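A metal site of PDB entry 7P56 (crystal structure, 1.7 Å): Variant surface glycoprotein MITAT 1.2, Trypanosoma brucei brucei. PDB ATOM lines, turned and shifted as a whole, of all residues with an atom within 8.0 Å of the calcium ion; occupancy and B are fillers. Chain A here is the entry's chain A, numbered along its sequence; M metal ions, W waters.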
ATOM      1  N   LYS A  30     -32.628 -13.432  -4.758  1.00  0.00           N
ATOM      2  CA  LYS A  30     -31.215 -13.254  -5.059  1.00  0.00           C
ATOM      3  C   LYS A  30     -30.620 -14.563  -5.542  1.00  0.00           C
ATOM      4  O   LYS A  30     -31.203 -15.641  -5.372  1.00  0.00           O
ATOM      5  CB  LYS A  30     -30.443 -12.728  -3.832  1.00  0.00           C
ATOM      6  CG  LYS A  30     -31.010 -11.451  -3.212  1.00  0.00           C
ATOM      7  CD  LYS A  30     -31.050 -10.286  -4.190  1.00  0.00           C
ATOM      8  CE  LYS A  30     -31.811  -9.096  -3.584  1.00  0.00           C
ATOM      9  NZ  LYS A  30     -31.975  -7.972  -4.556  1.00  0.00           N
ATOM     10  N   GLY A  31     -29.444 -14.445  -6.150  1.00  0.00           N
ATOM     11  CA  GLY A  31     -28.763 -15.608  -6.705  1.00  0.00           C
ATOM     12  C   GLY A  31     -28.486 -16.669  -5.656  1.00  0.00           C
ATOM     13  O   GLY A  31     -28.505 -16.415  -4.451  1.00  0.00           O
ATOM     14  N   LYS A  33     -26.579 -19.482  -3.538  1.00  0.00           N
ATOM     15  CA  LYS A  33     -25.305 -19.904  -2.982  1.00  0.00           C
ATOM     16  C   LYS A  33     -25.106 -21.414  -3.183  1.00  0.00           C
ATOM     17  O   LYS A  33     -26.038 -22.163  -3.519  1.00  0.00           O
ATOM     18  CB  LYS A  33     -25.220 -19.539  -1.505  1.00  0.00           C
ATOM     19  CG  LYS A  33     -25.273 -18.032  -1.239  1.00  0.00           C
ATOM     20  CD  LYS A  33     -25.055 -17.700   0.250  1.00  0.00           C
ATOM     21  CE  LYS A  33     -26.289 -18.091   1.081  1.00  0.00           C
ATOM     22  NZ  LYS A  33     -26.037 -17.888   2.553  1.00  0.00           N
ATOM     23  N   THR A 146     -19.406 -10.799  -9.313  1.00  0.00           N
ATOM     24  CA  THR A 146     -19.999 -10.816  -7.982  1.00  0.00           C
ATOM     25  C   THR A 146     -21.534 -10.810  -7.986  1.00  0.00           C
ATOM     26  O   THR A 146     -22.135 -10.715  -6.916  1.00  0.00           O
ATOM     27  CB  THR A 146     -19.504  -9.632  -7.140  1.00  0.00           C
ATOM     28  OG1 THR A 146     -19.845  -8.404  -7.802  1.00  0.00           O
ATOM     29  CG2 THR A 146     -17.990  -9.701  -6.950  1.00  0.00           C
ATOM     30  N   SER A 147     -22.178 -10.915  -9.157  1.00  0.00           N
ATOM     31  CA  SER A 147     -23.639 -10.852  -9.199  1.00  0.00           C
ATOM     32  C   SER A 147     -24.135 -11.771 -10.305  1.00  0.00           C
ATOM     33  O   SER A 147     -23.835 -11.558 -11.480  1.00  0.00           O
ATOM     34  CB  SER A 147     -24.118  -9.426  -9.433  1.00  0.00           C
ATOM     35  OG  SER A 147     -25.542  -9.391  -9.522  1.00  0.00           O
ATOM     36  N   MET A 151     -23.792 -18.775  -7.266  1.00  0.00           N
ATOM     37  CA  MET A 151     -22.827 -18.136  -6.385  1.00  0.00           C
ATOM     38  C   MET A 151     -22.073 -19.184  -5.574  1.00  0.00           C
ATOM     39  O   MET A 151     -22.520 -20.318  -5.403  1.00  0.00           O
ATOM     40  CB  MET A 151     -23.524 -17.149  -5.446  1.00  0.00           C
ATOM     41  CG  MET A 151     -24.315 -16.049  -6.164  1.00  0.00           C
ATOM     42  SD  MET A 151     -23.261 -14.867  -7.050  1.00  0.00           S
ATOM     43  CE  MET A 151     -22.350 -14.142  -5.689  1.00  0.00           C
ATOM     44  N   ASP A 152     -20.916 -18.765  -5.059  1.00  0.00           N
ATOM     45  CA  ASP A 152     -20.048 -19.639  -4.272  1.00  0.00           C
ATOM     46  C   ASP A 152     -20.666 -19.818  -2.873  1.00  0.00           C
ATOM     47  O   ASP A 152     -21.772 -19.374  -2.595  1.00  0.00           O
ATOM     48  CB  ASP A 152     -18.632 -19.073  -4.261  1.00  0.00           C
ATOM     49  CG  ASP A 152     -18.515 -17.697  -3.582  1.00  0.00           C
ATOM     50  OD1 ASP A 152     -19.375 -17.363  -2.733  1.00  0.00           O
ATOM     51  OD2 ASP A 152     -17.572 -16.934  -3.901  1.00  0.00           O
ATOM     52  N   SER A 154     -20.175 -18.574   0.075  1.00  0.00           N
ATOM     53  CA  SER A 154     -20.448 -17.408   0.885  1.00  0.00           C
ATOM     54  C   SER A 154     -21.274 -16.365   0.163  1.00  0.00           C
ATOM     55  O   SER A 154     -21.597 -15.321   0.753  1.00  0.00           O
ATOM     56  CB  SER A 154     -19.141 -16.756   1.356  1.00  0.00           C
ATOM     57  OG  SER A 154     -18.489 -16.150   0.260  1.00  0.00           O
ATOM     58  N   GLY A 155     -21.640 -16.604  -1.098  1.00  0.00           N
ATOM     59  CA  GLY A 155     -22.332 -15.582  -1.842  1.00  0.00           C
ATOM     60  C   GLY A 155     -21.456 -14.408  -2.231  1.00  0.00           C
ATOM     61  O   GLY A 155     -21.956 -13.300  -2.437  1.00  0.00           O
ATOM     62  N   THR A 156     -20.147 -14.632  -2.328  1.00  0.00           N
ATOM     63  CA  THR A 156     -19.213 -13.560  -2.637  1.00  0.00           C
ATOM     64  C   THR A 156     -19.065 -13.384  -4.145  1.00  0.00           C
ATOM     65  O   THR A 156     -19.339 -12.304  -4.681  1.00  0.00           O
ATOM     66  CB  THR A 156     -17.859 -13.837  -1.993  1.00  0.00           C
ATOM     67  OG1 THR A 156     -18.015 -13.856  -0.568  1.00  0.00           O
ATOM     68  CG2 THR A 156     -16.860 -12.739  -2.357  1.00  0.00           C
ATOM     69  N   ASN A 157     -18.664 -14.457  -4.848  1.00  0.00           N
ATOM     70  CA  ASN A 157     -18.404 -14.406  -6.276  1.00  0.00           C
ATOM     71  C   ASN A 157     -19.329 -15.355  -7.025  1.00  0.00           C
ATOM     72  O   ASN A 157     -19.782 -16.370  -6.482  1.00  0.00           O
ATOM     73  CB  ASN A 157     -16.954 -14.782  -6.585  1.00  0.00           C
ATOM     74  CG  ASN A 157     -15.949 -13.814  -5.968  1.00  0.00           C
ATOM     75  OD1 ASN A 157     -16.094 -12.597  -6.073  1.00  0.00           O
ATOM     76  ND2 ASN A 157     -14.946 -14.346  -5.327  1.00  0.00           N
ATOM     77  N   HIS A 207     -30.499 -18.430  -0.830  1.00  0.00           N
ATOM     78  CA  HIS A 207     -30.347 -17.153  -1.482  1.00  0.00           C
ATOM     79  C   HIS A 207     -29.220 -16.331  -0.866  1.00  0.00           C
ATOM     80  O   HIS A 207     -29.064 -16.262   0.361  1.00  0.00           O
ATOM     81  CB  HIS A 207     -31.649 -16.362  -1.413  1.00  0.00           C
ATOM     82  CG  HIS A 207     -32.779 -16.967  -2.188  1.00  0.00           C
ATOM     83  ND1 HIS A 207     -32.937 -16.802  -3.538  1.00  0.00           N
ATOM     84  CD2 HIS A 207     -33.842 -17.702  -1.776  1.00  0.00           C
ATOM     85  CE1 HIS A 207     -34.030 -17.434  -3.946  1.00  0.00           C
ATOM     86  NE2 HIS A 207     -34.595 -17.981  -2.886  1.00  0.00           N
ATOM     87  N   ASP A 208     -28.433 -15.696  -1.738  1.00  0.00           N
ATOM     88  CA  ASP A 208     -27.433 -14.709  -1.354  1.00  0.00           C
ATOM     89  C   ASP A 208     -28.113 -13.430  -0.830  1.00  0.00           C
ATOM     90  O   ASP A 208     -29.328 -13.248  -0.931  1.00  0.00           O
ATOM     91  CB  ASP A 208     -26.520 -14.408  -2.538  1.00  0.00           C
ATOM     92  CG  ASP A 208     -25.403 -13.462  -2.191  1.00  0.00           C
ATOM     93  OD1 ASP A 208     -24.716 -13.711  -1.176  1.00  0.00           O
ATOM     94  OD2 ASP A 208     -25.225 -12.467  -2.917  1.00  0.00           O
ATOM     95  N   ASN A 209     -27.302 -12.518  -0.284  1.00  0.00           N
ATOM     96  CA  ASN A 209     -27.849 -11.255   0.202  1.00  0.00           C
ATOM     97  C   ASN A 209     -28.030 -10.226  -0.905  1.00  0.00           C
ATOM     98  O   ASN A 209     -28.961  -9.422  -0.838  1.00  0.00           O
ATOM     99  CB  ASN A 209     -26.957 -10.687   1.301  1.00  0.00           C
ATOM    100  CG  ASN A 209     -25.575 -10.319   0.793  1.00  0.00           C
ATOM    101  OD1 ASN A 209     -24.929 -11.106   0.100  1.00  0.00           O
ATOM    102  ND2 ASN A 209     -25.131  -9.120   1.126  1.00  0.00           N
ATOM    103  N   ASP A 210     -27.168 -10.214  -1.939  1.00  0.00           N
ATOM    104  CA  ASP A 210     -27.257  -9.143  -2.936  1.00  0.00           C
ATOM    105  C   ASP A 210     -27.085  -9.565  -4.389  1.00  0.00           C
ATOM    106  O   ASP A 210     -27.398  -8.756  -5.274  1.00  0.00           O
ATOM    107  CB  ASP A 210     -26.241  -8.019  -2.630  1.00  0.00           C
ATOM    108  CG  ASP A 210     -24.850  -8.533  -2.271  1.00  0.00           C
ATOM    109  OD1 ASP A 210     -24.529  -9.709  -2.540  1.00  0.00           O
ATOM    110  OD2 ASP A 210     -24.065  -7.749  -1.705  1.00  0.00           O
ATOM    111  N   ALA A 211     -26.620 -10.778  -4.692  1.00  0.00           N
ATOM    112  CA  ALA A 211     -26.474 -11.211  -6.070  1.00  0.00           C
ATOM    113  C   ALA A 211     -27.816 -11.164  -6.800  1.00  0.00           C
ATOM    114  O   ALA A 211     -28.819 -11.705  -6.325  1.00  0.00           O
ATOM    115  CB  ALA A 211     -25.902 -12.627  -6.107  1.00  0.00           C
ATOM    116  N   GLU A 212     -27.846 -10.551  -7.977  1.00  0.00           N
ATOM    117  CA  GLU A 212     -29.081 -10.430  -8.737  1.00  0.00           C
ATOM    118  C   GLU A 212     -29.274 -11.616  -9.680  1.00  0.00           C
ATOM    119  O   GLU A 212     -28.344 -12.029 -10.378  1.00  0.00           O
ATOM    120  CB  GLU A 212     -29.095  -9.118  -9.517  1.00  0.00           C
ATOM    121  CG  GLU A 212     -29.159  -7.929  -8.587  1.00  0.00           C
ATOM    122  CD  GLU A 212     -29.105  -6.618  -9.328  1.00  0.00           C
ATOM    123  OE1 GLU A 212     -28.599  -6.610 -10.462  1.00  0.00           O
ATOM    124  OE2 GLU A 212     -29.571  -5.594  -8.787  1.00  0.00           O
HETATM  125 CA    CA M   1     -23.313 -11.584  -1.710  1.00  0.00          CA
HETATM  126  O   HOH W   1     -22.222 -12.718   0.417  1.00  0.00           O
HETATM  127  O   HOH W   2     -22.153 -10.811  -3.887  1.00  0.00           O
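The nearest printed residue that does not touch the calcium ion is Thr 156 (4.4 Å).
The calcium ion is bound by the backbone carbonyl oxygen (O) of Gly 155 (2.3 Å). The calcium ion is bound by the side-chain carboxylate (OD1) of Asp 210, 2.4 Å away. The calcium ion is bound by the side-chain carboxylate (OD2) of Asp 208, 2.4 Å away. OD1 of Asn 209 is bound to the calcium ion, 2.5 Å away. The calcium ion is bound by water W2 (2.6 Å). The side-chain carboxylate (OD1) of Asp 208 binds the calcium ion (2.6 Å). The calcium ion is bound by water W1 (2.6 Å). The calcium ion has seven donor atoms within binding distance.
The backbone NH of Asp 208 sits at hydrogen-bond distance from the backbone carbonyl oxygen of Gly 31, 2.8 Å away. N of Gly 155 sits at hydrogen-bond distance from OD1 of Asp 152, at 2.9 Å. The side-chain carboxylate of Asp 208 sits close to the backbone NH of Ala 211, at 2.8 Å.
Water W2 lies within hydrogen-bond range of O of Thr 146 (3.0 Å) and O of Thr 156 (3.3 Å).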
